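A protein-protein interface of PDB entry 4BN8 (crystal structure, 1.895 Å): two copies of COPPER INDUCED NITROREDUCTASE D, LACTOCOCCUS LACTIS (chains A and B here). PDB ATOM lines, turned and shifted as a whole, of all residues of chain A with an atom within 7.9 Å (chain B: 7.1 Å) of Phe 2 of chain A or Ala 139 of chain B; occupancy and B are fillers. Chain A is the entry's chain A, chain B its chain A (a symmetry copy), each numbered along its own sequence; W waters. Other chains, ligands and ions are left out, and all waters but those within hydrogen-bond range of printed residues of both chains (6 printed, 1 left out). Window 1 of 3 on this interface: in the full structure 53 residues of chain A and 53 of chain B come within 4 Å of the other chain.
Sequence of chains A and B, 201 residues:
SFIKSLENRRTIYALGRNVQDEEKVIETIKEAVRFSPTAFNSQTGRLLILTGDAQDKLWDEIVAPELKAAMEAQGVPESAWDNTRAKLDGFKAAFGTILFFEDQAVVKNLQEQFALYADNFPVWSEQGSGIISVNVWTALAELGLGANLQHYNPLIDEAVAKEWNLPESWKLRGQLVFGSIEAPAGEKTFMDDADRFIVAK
The backbone NH of Phe 2 of chain A lies within hydrogen-bond range of the side-chain carboxylate of Glu 142 of chain B (2.9 Å).
The side-chain hydroxyl of Ser 1 of chain A lies close to the backbone NH of Lys 4 of chain A (3.2 Å).
OG of Ser 5 of chain B is in hydrogen-bond range of O of Ser 1 of chain B (3.2 Å).
The backbone carbonyl oxygen of Ser 1 of chain A lies within hydrogen-bond range of the side-chain hydroxyl of Ser 5 of chain A, at 3.2 Å.
O of Val 134 of chain B sits at hydrogen-bond distance from OG1 of Thr 138 of chain B.
Among the printed residues, merely in contact across the chains: Asn 135 of chain A with Phe 2 of chain B, Phe 2 of chain A with Asn 135 of chain B, Phe 2 of chain A with Thr 138 of chain B, Thr 138 of chain A with Phe 2 of chain B, Phe 2 of chain A with Phe 2 of chain B, Asn 135 of chain A with Leu 6 of chain B, Leu 6 of chain A with Asn 135 of chain B, Ser 1 of chain A with Glu 142 of chain B, Phe 2 of chain A with Ala 139 of chain B, Ile 3 of chain A with Glu 31 of chain B, Leu 6 of chain A with Ala 32 of chain B, Phe 2 of chain A with Ser 5 of chain B, Ser 5 of chain A with Phe 2 of chain B and Ile 3 of chain A with Ala 32 of chain B.
Printed residues of chain A within 4 Å of Leu 6 of chain B: Asn 135 (3.6 Å).
Of the printed residues of chain A, Ser 5 of chain B touches Phe 2 (3.8 Å).
Printed residues of chain A within 4 Å of Thr 138 of chain B: Phe 2.
Printed residues of chain A within 4 Å of Ala 32 of chain B: Ile 3 (3.97 Å) and Leu 6 (3.8 Å).
Ile 29 of chain B touches none of the printed residues of chain A.
The nearest printed residue of chain B that does not touch Phe 2 of chain A is Leu 6 of chain B (4.8 Å).
The nearest residue of chain A that does not touch Ala 139 of chain B is Ile 3 of chain A (4.04 Å).
Among the printed residues, no Asp or Glu carboxylate lies within 4 Å of a Lys or Arg side-chain nitrogen of the other chain.
Phe 2 of chain B touches its own counterpart, Phe 2 of chain A.
Phe 2 of chain A touches Asn 135 of chain B, and with the chains exchanged Asn 135 of chain A touches Phe 2 of chain B.
Phe 2 of chain A touches Thr 138 of chain B, and with the chains exchanged Thr 138 of chain A touches Phe 2 of chain B.
Leu 6 of chain A touches Asn 135 of chain B, and with the chains exchanged Asn 135 of chain A touches Leu 6 of chain B.
Positions printed for both chains: 1, 2, 5, 6, 135 and 138.
Of the 15 pairs that touch across the chains among the printed residues, 9 have their exchanged pair printed and touching as well.
Water W3 lies within hydrogen-bond range of the side-chain carboxylate of Glu 142 of chain B (2.4 Å), the side-chain hydroxyl of Ser 1 of chain A (2.8 Å), the backbone NH of Ile 3 of chain A (3.1 Å) and the backbone NH of Phe 2 of chain A (3.2 Å).
Water W5 lies within hydrogen-bond range of OD1 of Asn 135 of chain B (2.8 Å), OD1 of Asn 135 of chain A (2.9 Å) and OG1 of Thr 138 of chain A (3.3 Å).
Water W2 lies within hydrogen-bond range of the side-chain amide oxygen (OD1) of Asn 135 of chain A (2.8 Å), the side-chain amide oxygen (OD1) of Asn 135 of chain B (2.9 Å) and the side-chain hydroxyl (OG1) of Thr 138 of chain B (3.3 Å).
Water W1 bridges the side-chain amide nitrogen (ND2) of Asn 135 of chain B (3.0 Å) and the side-chain hydroxyl (OG1) of Thr 138 of chain A (3.3 Å).
Water W4 bridges the side-chain amide nitrogen of Asn 135 of chain A (3.0 Å) and the side-chain hydroxyl of Thr 138 of chain B (3.3 Å).
Water W6 lies within hydrogen-bond range of the side-chain hydroxyl of Ser 5 of chain A (3.1 Å) and the side-chain hydroxyl of Ser 5 of chain B (3.1 Å).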
ATOM      1  N   SER A   1      20.618  -2.128 -28.423  1.00  0.00           N
ATOM      2  CA  SER A   1      20.609  -2.009 -26.971  1.00  0.00           C
ATOM      3  C   SER A   1      20.774  -3.381 -26.347  1.00  0.00           C
ATOM      4  O   SER A   1      19.988  -4.293 -26.598  1.00  0.00           O
ATOM      5  CB  SER A   1      19.302  -1.369 -26.493  1.00  0.00           C
ATOM      6  OG  SER A   1      19.141  -1.466 -25.080  1.00  0.00           O
ATOM      7  N   PHE A   2      21.807  -3.519 -25.525  1.00  0.00           N
ATOM      8  CA  PHE A   2      22.079  -4.779 -24.859  1.00  0.00           C
ATOM      9  C   PHE A   2      20.998  -5.111 -23.832  1.00  0.00           C
ATOM     10  O   PHE A   2      20.554  -6.252 -23.732  1.00  0.00           O
ATOM     11  CB  PHE A   2      23.455  -4.734 -24.193  1.00  0.00           C
ATOM     12  CG  PHE A   2      23.751  -5.940 -23.367  1.00  0.00           C
ATOM     13  CD1 PHE A   2      24.091  -7.134 -23.969  1.00  0.00           C
ATOM     14  CD2 PHE A   2      23.673  -5.887 -21.986  1.00  0.00           C
ATOM     15  CE1 PHE A   2      24.350  -8.256 -23.206  1.00  0.00           C
ATOM     16  CE2 PHE A   2      23.934  -7.006 -21.222  1.00  0.00           C
ATOM     17  CZ  PHE A   2      24.269  -8.190 -21.834  1.00  0.00           C
ATOM     18  N   ILE A   3      20.579  -4.116 -23.061  1.00  0.00           N
ATOM     19  CA  ILE A   3      19.491  -4.315 -22.113  1.00  0.00           C
ATOM     20  C   ILE A   3      18.229  -4.824 -22.825  1.00  0.00           C
ATOM     21  O   ILE A   3      17.576  -5.755 -22.351  1.00  0.00           O
ATOM     22  CB  ILE A   3      19.178  -3.026 -21.334  1.00  0.00           C
ATOM     23  CG1 ILE A   3      20.380  -2.622 -20.471  1.00  0.00           C
ATOM     24  CG2 ILE A   3      17.957  -3.220 -20.455  1.00  0.00           C
ATOM     25  CD1 ILE A   3      20.820  -3.701 -19.502  1.00  0.00           C
ATOM     26  N   LYS A   4      17.889  -4.228 -23.965  1.00  0.00           N
ATOM     27  CA  LYS A   4      16.733  -4.683 -24.735  1.00  0.00           C
ATOM     28  C   LYS A   4      16.912  -6.129 -25.187  1.00  0.00           C
ATOM     29  O   LYS A   4      15.959  -6.901 -25.192  1.00  0.00           O
ATOM     30  CB  LYS A   4      16.488  -3.792 -25.956  1.00  0.00           C
ATOM     31  CG  LYS A   4      15.528  -2.629 -25.715  1.00  0.00           C
ATOM     32  CD  LYS A   4      16.244  -1.373 -25.224  1.00  0.00           C
ATOM     33  CE  LYS A   4      15.276  -0.212 -25.008  1.00  0.00           C
ATOM     34  NZ  LYS A   4      14.348  -0.431 -23.865  1.00  0.00           N
ATOM     35  N   SER A   5      18.131  -6.501 -25.564  1.00  0.00           N
ATOM     36  CA  SER A   5      18.391  -7.876 -25.970  1.00  0.00           C
ATOM     37  C   SER A   5      18.111  -8.825 -24.818  1.00  0.00           C
ATOM     38  O   SER A   5      17.492  -9.871 -25.009  1.00  0.00           O
ATOM     39  CB  SER A   5      19.828  -8.046 -26.464  1.00  0.00           C
ATOM     40  OG  SER A   5      20.041  -7.288 -27.641  1.00  0.00           O
ATOM     41  N   LEU A   6      18.567  -8.458 -23.623  1.00  0.00           N
ATOM     42  CA  LEU A   6      18.308  -9.262 -22.438  1.00  0.00           C
ATOM     43  C   LEU A   6      16.807  -9.400 -22.239  1.00  0.00           C
ATOM     44  O   LEU A   6      16.302 -10.490 -21.991  1.00  0.00           O
ATOM     45  CB  LEU A   6      18.931  -8.628 -21.191  1.00  0.00           C
ATOM     46  CG  LEU A   6      20.459  -8.594 -21.090  1.00  0.00           C
ATOM     47  CD1 LEU A   6      20.878  -8.036 -19.741  1.00  0.00           C
ATOM     48  CD2 LEU A   6      21.057  -9.968 -21.307  1.00  0.00           C
ATOM     49  N   GLU A   7      16.087  -8.292 -22.351  1.00  0.00           N
ATOM     50  CA  GLU A   7      14.655  -8.327 -22.099  1.00  0.00           C
ATOM     51  C   GLU A   7      13.912  -9.155 -23.146  1.00  0.00           C
ATOM     52  O   GLU A   7      12.872  -9.733 -22.849  1.00  0.00           O
ATOM     53  CB  GLU A   7      14.079  -6.914 -22.024  1.00  0.00           C
ATOM     54  CG  GLU A   7      12.657  -6.897 -21.501  1.00  0.00           C
ATOM     55  CD  GLU A   7      12.129  -5.500 -21.286  1.00  0.00           C
ATOM     56  OE1 GLU A   7      12.869  -4.538 -21.577  1.00  0.00           O
ATOM     57  OE2 GLU A   7      10.976  -5.370 -20.826  1.00  0.00           O
ATOM     58  N   ASN A   8      14.450  -9.235 -24.359  1.00  0.00           N
ATOM     59  CA  ASN A   8      13.812  -9.977 -25.445  1.00  0.00           C
ATOM     60  C   ASN A   8      13.895 -11.484 -25.246  1.00  0.00           C
ATOM     61  O   ASN A   8      13.081 -12.239 -25.778  1.00  0.00           O
ATOM     62  CB  ASN A   8      14.423  -9.604 -26.799  1.00  0.00           C
ATOM     63  CG  ASN A   8      13.938  -8.263 -27.310  1.00  0.00           C
ATOM     64  OD1 ASN A   8      12.931  -7.739 -26.847  1.00  0.00           O
ATOM     65  ND2 ASN A   8      14.656  -7.703 -28.277  1.00  0.00           N
ATOM     66  N   ASN A 135      23.860 -16.819 -22.746  1.00  0.00           N
ATOM     67  CA  ASN A 135      24.357 -16.055 -23.884  1.00  0.00           C
ATOM     68  C   ASN A 135      23.839 -16.643 -25.205  1.00  0.00           C
ATOM     69  O   ASN A 135      23.407 -15.905 -26.089  1.00  0.00           O
ATOM     70  CB  ASN A 135      25.888 -15.940 -23.863  1.00  0.00           C
ATOM     71  CG  ASN A 135      26.378 -14.786 -22.977  1.00  0.00           C
ATOM     72  OD1 ASN A 135      25.592 -13.927 -22.564  1.00  0.00           O
ATOM     73  ND2 ASN A 135      27.683 -14.757 -22.700  1.00  0.00           N
ATOM     74  N   THR A 138      20.055 -15.952 -25.424  1.00  0.00           N
ATOM     75  CA  THR A 138      19.793 -14.563 -25.780  1.00  0.00           C
ATOM     76  C   THR A 138      20.128 -14.274 -27.243  1.00  0.00           C
ATOM     77  O   THR A 138      19.415 -13.531 -27.906  1.00  0.00           O
ATOM     78  CB  THR A 138      20.563 -13.582 -24.854  1.00  0.00           C
ATOM     79  OG1 THR A 138      20.222 -13.842 -23.485  1.00  0.00           O
ATOM     80  CG2 THR A 138      20.215 -12.146 -25.175  1.00  0.00           C
ATOM     81  N   SER B   1      23.752  -5.191 -32.261  1.00  0.00           N
ATOM     82  CA  SER B   1      24.122  -6.594 -32.394  1.00  0.00           C
ATOM     83  C   SER B   1      24.500  -7.152 -31.035  1.00  0.00           C
ATOM     84  O   SER B   1      25.400  -6.645 -30.368  1.00  0.00           O
ATOM     85  CB  SER B   1      25.293  -6.751 -33.369  1.00  0.00           C
ATOM     86  OG  SER B   1      25.850  -8.062 -33.334  1.00  0.00           O
ATOM     87  N   PHE B   2      23.803  -8.206 -30.631  1.00  0.00           N
ATOM     88  CA  PHE B   2      24.064  -8.839 -29.352  1.00  0.00           C
ATOM     89  C   PHE B   2      25.430  -9.521 -29.336  1.00  0.00           C
ATOM     90  O   PHE B   2      26.170  -9.427 -28.359  1.00  0.00           O
ATOM     91  CB  PHE B   2      22.959  -9.845 -29.029  1.00  0.00           C
ATOM     92  CG  PHE B   2      23.226 -10.642 -27.797  1.00  0.00           C
ATOM     93  CD1 PHE B   2      23.063 -10.076 -26.549  1.00  0.00           C
ATOM     94  CD2 PHE B   2      23.659 -11.954 -27.884  1.00  0.00           C
ATOM     95  CE1 PHE B   2      23.326 -10.807 -25.407  1.00  0.00           C
ATOM     96  CE2 PHE B   2      23.919 -12.687 -26.743  1.00  0.00           C
ATOM     97  CZ  PHE B   2      23.756 -12.111 -25.507  1.00  0.00           C
ATOM     98  N   SER B   5      27.982  -7.009 -28.756  1.00  0.00           N
ATOM     99  CA  SER B   5      27.994  -6.600 -27.359  1.00  0.00           C
ATOM    100  C   SER B   5      28.815  -7.575 -26.533  1.00  0.00           C
ATOM    101  O   SER B   5      29.612  -7.161 -25.692  1.00  0.00           O
ATOM    102  CB  SER B   5      26.574  -6.492 -26.800  1.00  0.00           C
ATOM    103  OG  SER B   5      25.859  -5.464 -27.459  1.00  0.00           O
ATOM    104  N   LEU B   6      28.620  -8.868 -26.775  1.00  0.00           N
ATOM    105  CA  LEU B   6      29.393  -9.890 -26.084  1.00  0.00           C
ATOM    106  C   LEU B   6      30.873  -9.676 -26.360  1.00  0.00           C
ATOM    107  O   LEU B   6      31.695  -9.712 -25.451  1.00  0.00           O
ATOM    108  CB  LEU B   6      28.987 -11.294 -26.539  1.00  0.00           C
ATOM    109  CG  LEU B   6      27.591 -11.796 -26.159  1.00  0.00           C
ATOM    110  CD1 LEU B   6      27.421 -13.241 -26.596  1.00  0.00           C
ATOM    111  CD2 LEU B   6      27.340 -11.658 -24.671  1.00  0.00           C
ATOM    112  N   ARG B   9      32.699  -6.845 -24.426  1.00  0.00           N
ATOM    113  CA  ARG B   9      33.008  -7.079 -23.022  1.00  0.00           C
ATOM    114  C   ARG B   9      34.351  -7.764 -22.904  1.00  0.00           C
ATOM    115  O   ARG B   9      34.569  -8.818 -23.508  1.00  0.00           O
ATOM    116  CB  ARG B   9      31.950  -7.956 -22.363  1.00  0.00           C
ATOM    117  CG  ARG B   9      32.170  -8.154 -20.871  1.00  0.00           C
ATOM    118  CD  ARG B   9      31.894  -9.588 -20.445  1.00  0.00           C
ATOM    119  NE  ARG B   9      32.615 -10.543 -21.285  1.00  0.00           N
ATOM    120  CZ  ARG B   9      33.886 -10.901 -21.114  1.00  0.00           C
ATOM    121  NH1 ARG B   9      34.609 -10.402 -20.116  1.00  0.00           N
ATOM    122  NH2 ARG B   9      34.435 -11.776 -21.943  1.00  0.00           N
ATOM    123  N   THR B  28      21.573   0.705 -15.149  1.00  0.00           N
ATOM    124  CA  THR B  28      21.941  -0.357 -16.079  1.00  0.00           C
ATOM    125  C   THR B  28      22.324  -1.630 -15.334  1.00  0.00           C
ATOM    126  O   THR B  28      22.006  -2.739 -15.779  1.00  0.00           O
ATOM    127  CB  THR B  28      23.098   0.091 -16.997  1.00  0.00           C
ATOM    128  OG1 THR B  28      22.745   1.322 -17.643  1.00  0.00           O
ATOM    129  CG2 THR B  28      23.370  -0.948 -18.058  1.00  0.00           C
ATOM    130  N   ILE B  29      23.005  -1.480 -14.201  1.00  0.00           N
ATOM    131  CA  ILE B  29      23.362  -2.635 -13.383  1.00  0.00           C
ATOM    132  C   ILE B  29      22.088  -3.346 -12.928  1.00  0.00           C
ATOM    133  O   ILE B  29      21.983  -4.570 -13.014  1.00  0.00           O
ATOM    134  CB  ILE B  29      24.187  -2.236 -12.145  1.00  0.00           C
ATOM    135  CG1 ILE B  29      25.600  -1.785 -12.550  1.00  0.00           C
ATOM    136  CG2 ILE B  29      24.288  -3.400 -11.182  1.00  0.00           C
ATOM    137  CD1 ILE B  29      26.315  -1.001 -11.459  1.00  0.00           C
ATOM    138  N   GLU B  31      19.051  -3.224 -14.258  1.00  0.00           N
ATOM    139  CA  GLU B  31      18.319  -3.795 -15.385  1.00  0.00           C
ATOM    140  C   GLU B  31      18.930  -5.111 -15.853  1.00  0.00           C
ATOM    141  O   GLU B  31      18.215  -6.045 -16.210  1.00  0.00           O
ATOM    142  CB  GLU B  31      18.264  -2.810 -16.552  1.00  0.00           C
ATOM    143  CG  GLU B  31      17.297  -1.658 -16.345  1.00  0.00           C
ATOM    144  CD  GLU B  31      17.001  -0.900 -17.626  1.00  0.00           C
ATOM    145  OE1 GLU B  31      17.936  -0.309 -18.205  1.00  0.00           O
ATOM    146  OE2 GLU B  31      15.830  -0.905 -18.059  1.00  0.00           O
ATOM    147  N   ALA B  32      20.256  -5.177 -15.860  1.00  0.00           N
ATOM    148  CA  ALA B  32      20.952  -6.364 -16.332  1.00  0.00           C
ATOM    149  C   ALA B  32      20.631  -7.547 -15.430  1.00  0.00           C
ATOM    150  O   ALA B  32      20.411  -8.658 -15.909  1.00  0.00           O
ATOM    151  CB  ALA B  32      22.458  -6.119 -16.393  1.00  0.00           C
ATOM    152  N   SER B 133      26.413 -11.933 -13.172  1.00  0.00           N
ATOM    153  CA  SER B 133      27.726 -11.282 -13.175  1.00  0.00           C
ATOM    154  C   SER B 133      28.126 -10.832 -14.584  1.00  0.00           C
ATOM    155  O   SER B 133      28.521  -9.682 -14.783  1.00  0.00           O
ATOM    156  CB  SER B 133      28.795 -12.203 -12.588  1.00  0.00           C
ATOM    157  OG  SER B 133      28.570 -12.445 -11.209  1.00  0.00           O
ATOM    158  N   VAL B 134      28.002 -11.722 -15.570  1.00  0.00           N
ATOM    159  CA  VAL B 134      28.432 -11.388 -16.927  1.00  0.00           C
ATOM    160  C   VAL B 134      27.442 -10.493 -17.657  1.00  0.00           C
ATOM    161  O   VAL B 134      27.830  -9.740 -18.551  1.00  0.00           O
ATOM    162  CB  VAL B 134      28.690 -12.632 -17.793  1.00  0.00           C
ATOM    163  CG1 VAL B 134      29.748 -13.506 -17.154  1.00  0.00           C
ATOM    164  CG2 VAL B 134      27.392 -13.399 -18.033  1.00  0.00           C
ATOM    165  N   ASN B 135      26.161 -10.576 -17.302  1.00  0.00           N
ATOM    166  CA  ASN B 135      25.192  -9.659 -17.891  1.00  0.00           C
ATOM    167  C   ASN B 135      25.468  -8.214 -17.452  1.00  0.00           C
ATOM    168  O   ASN B 135      25.434  -7.296 -18.270  1.00  0.00           O
ATOM    169  CB  ASN B 135      23.749 -10.091 -17.587  1.00  0.00           C
ATOM    170  CG  ASN B 135      23.232 -11.146 -18.574  1.00  0.00           C
ATOM    171  OD1 ASN B 135      23.845 -11.392 -19.618  1.00  0.00           O
ATOM    172  ND2 ASN B 135      22.091 -11.759 -18.252  1.00  0.00           N
ATOM    173  N   VAL B 136      25.758  -8.015 -16.172  1.00  0.00           N
ATOM    174  CA  VAL B 136      26.158  -6.695 -15.684  1.00  0.00           C
ATOM    175  C   VAL B 136      27.473  -6.243 -16.350  1.00  0.00           C
ATOM    176  O   VAL B 136      27.579  -5.128 -16.868  1.00  0.00           O
ATOM    177  CB  VAL B 136      26.328  -6.704 -14.149  1.00  0.00           C
ATOM    178  CG1 VAL B 136      26.981  -5.408 -13.663  1.00  0.00           C
ATOM    179  CG2 VAL B 136      24.981  -6.937 -13.465  1.00  0.00           C
ATOM    180  N   TRP B 137      28.460  -7.128 -16.338  1.00  0.00           N
ATOM    181  CA  TRP B 137      29.763  -6.878 -16.948  1.00  0.00           C
ATOM    182  C   TRP B 137      29.582  -6.370 -18.380  1.00  0.00           C
ATOM    183  O   TRP B 137      30.181  -5.371 -18.779  1.00  0.00           O
ATOM    184  CB  TRP B 137      30.545  -8.195 -16.936  1.00  0.00           C
ATOM    185  CG  TRP B 137      32.025  -8.111 -17.142  1.00  0.00           C
ATOM    186  CD1 TRP B 137      32.748  -7.055 -17.620  1.00  0.00           C
ATOM    187  CD2 TRP B 137      32.964  -9.152 -16.871  1.00  0.00           C
ATOM    188  NE1 TRP B 137      34.083  -7.383 -17.665  1.00  0.00           N
ATOM    189  CE2 TRP B 137      34.240  -8.667 -17.209  1.00  0.00           C
ATOM    190  CE3 TRP B 137      32.848 -10.456 -16.379  1.00  0.00           C
ATOM    191  CZ2 TRP B 137      35.391  -9.437 -17.065  1.00  0.00           C
ATOM    192  CZ3 TRP B 137      33.991 -11.216 -16.241  1.00  0.00           C
ATOM    193  CH2 TRP B 137      35.245 -10.705 -16.577  1.00  0.00           C
ATOM    194  N   THR B 138      28.730  -7.050 -19.140  1.00  0.00           N
ATOM    195  CA  THR B 138      28.510  -6.726 -20.545  1.00  0.00           C
ATOM    196  C   THR B 138      27.727  -5.425 -20.716  1.00  0.00           C
ATOM    197  O   THR B 138      28.012  -4.646 -21.618  1.00  0.00           O
ATOM    198  CB  THR B 138      27.789  -7.884 -21.289  1.00  0.00           C
ATOM    199  OG1 THR B 138      28.544  -9.094 -21.146  1.00  0.00           O
ATOM    200  CG2 THR B 138      27.645  -7.574 -22.763  1.00  0.00           C
ATOM    201  N   ALA B 139      26.750  -5.180 -19.847  1.00  0.00           N
ATOM    202  CA  ALA B 139      25.982  -3.943 -19.910  1.00  0.00           C
ATOM    203  C   ALA B 139      26.876  -2.727 -19.610  1.00  0.00           C
ATOM    204  O   ALA B 139      26.751  -1.679 -20.243  1.00  0.00           O
ATOM    205  CB  ALA B 139      24.806  -3.999 -18.942  1.00  0.00           C
ATOM    206  N   LEU B 140      27.776  -2.870 -18.645  1.00  0.00           N
ATOM    207  CA  LEU B 140      28.735  -1.811 -18.332  1.00  0.00           C
ATOM    208  C   LEU B 140      29.645  -1.522 -19.521  1.00  0.00           C
ATOM    209  O   LEU B 140      29.971  -0.366 -19.801  1.00  0.00           O
ATOM    210  CB  LEU B 140      29.585  -2.204 -17.129  1.00  0.00           C
ATOM    211  CG  LEU B 140      28.864  -2.291 -15.782  1.00  0.00           C
ATOM    212  CD1 LEU B 140      29.774  -2.905 -14.738  1.00  0.00           C
ATOM    213  CD2 LEU B 140      28.415  -0.927 -15.332  1.00  0.00           C
ATOM    214  N   ALA B 141      30.065  -2.581 -20.208  1.00  0.00           N
ATOM    215  CA  ALA B 141      30.927  -2.444 -21.376  1.00  0.00           C
ATOM    216  C   ALA B 141      30.222  -1.675 -22.487  1.00  0.00           C
ATOM    217  O   ALA B 141      30.854  -0.915 -23.214  1.00  0.00           O
ATOM    218  CB  ALA B 141      31.372  -3.820 -21.875  1.00  0.00           C
ATOM    219  N   GLU B 142      28.915  -1.875 -22.636  1.00  0.00           N
ATOM    220  CA  GLU B 142      28.156  -1.130 -23.631  1.00  0.00           C
ATOM    221  C   GLU B 142      28.149   0.362 -23.312  1.00  0.00           C
ATOM    222  O   GLU B 142      28.057   1.194 -24.206  1.00  0.00           O
ATOM    223  CB  GLU B 142      26.722  -1.640 -23.729  1.00  0.00           C
ATOM    224  CG  GLU B 142      25.862  -0.798 -24.654  1.00  0.00           C
ATOM    225  CD  GLU B 142      24.428  -1.260 -24.690  1.00  0.00           C
ATOM    226  OE1 GLU B 142      23.756  -1.215 -23.639  1.00  0.00           O
ATOM    227  OE2 GLU B 142      23.979  -1.674 -25.774  1.00  0.00           O
ATOM    228  N   LEU B 143      28.246   0.698 -22.029  1.00  0.00           N
ATOM    229  CA  LEU B 143      28.319   2.103 -21.623  1.00  0.00           C
ATOM    230  C   LEU B 143      29.721   2.683 -21.798  1.00  0.00           C
ATOM    231  O   LEU B 143      29.939   3.865 -21.533  1.00  0.00           O
ATOM    232  CB  LEU B 143      27.904   2.267 -20.165  1.00  0.00           C
ATOM    233  CG  LEU B 143      26.442   1.963 -19.843  1.00  0.00           C
ATOM    234  CD1 LEU B 143      26.181   2.215 -18.370  1.00  0.00           C
ATOM    235  CD2 LEU B 143      25.505   2.793 -20.709  1.00  0.00           C
ATOM    236  N   GLY B 144      30.669   1.853 -22.229  1.00  0.00           N
ATOM    237  CA  GLY B 144      32.033   2.305 -22.428  1.00  0.00           C
ATOM    238  C   GLY B 144      32.914   2.107 -21.206  1.00  0.00           C
ATOM    239  O   GLY B 144      34.075   2.514 -21.200  1.00  0.00           O
ATOM    240  N   LEU B 145      32.366   1.470 -20.175  1.00  0.00           N
ATOM    241  CA  LEU B 145      33.114   1.207 -18.950  1.00  0.00           C
ATOM    242  C   LEU B 145      33.758  -0.173 -18.968  1.00  0.00           C
ATOM    243  O   LEU B 145      33.193  -1.123 -19.495  1.00  0.00           O
ATOM    244  CB  LEU B 145      32.185   1.304 -17.743  1.00  0.00           C
ATOM    245  CG  LEU B 145      31.555   2.673 -17.495  1.00  0.00           C
ATOM    246  CD1 LEU B 145      30.712   2.623 -16.233  1.00  0.00           C
ATOM    247  CD2 LEU B 145      32.632   3.746 -17.393  1.00  0.00           C
HETATM  248  O   HOH W   1      20.541 -13.476 -20.234  1.00  0.00           O
HETATM  249  O   HOH W   2      26.216 -11.458 -21.293  1.00  0.00           O
HETATM  250  O   HOH W   3      21.320  -1.136 -23.395  1.00  0.00           O
HETATM  251  O   HOH W   4      29.034 -12.331 -21.446  1.00  0.00           O
HETATM  252  O   HOH W   5      22.961 -12.936 -21.839  1.00  0.00           O
HETATM  253  O   HOH W   6      22.820  -5.915 -28.024  1.00  0.00           O
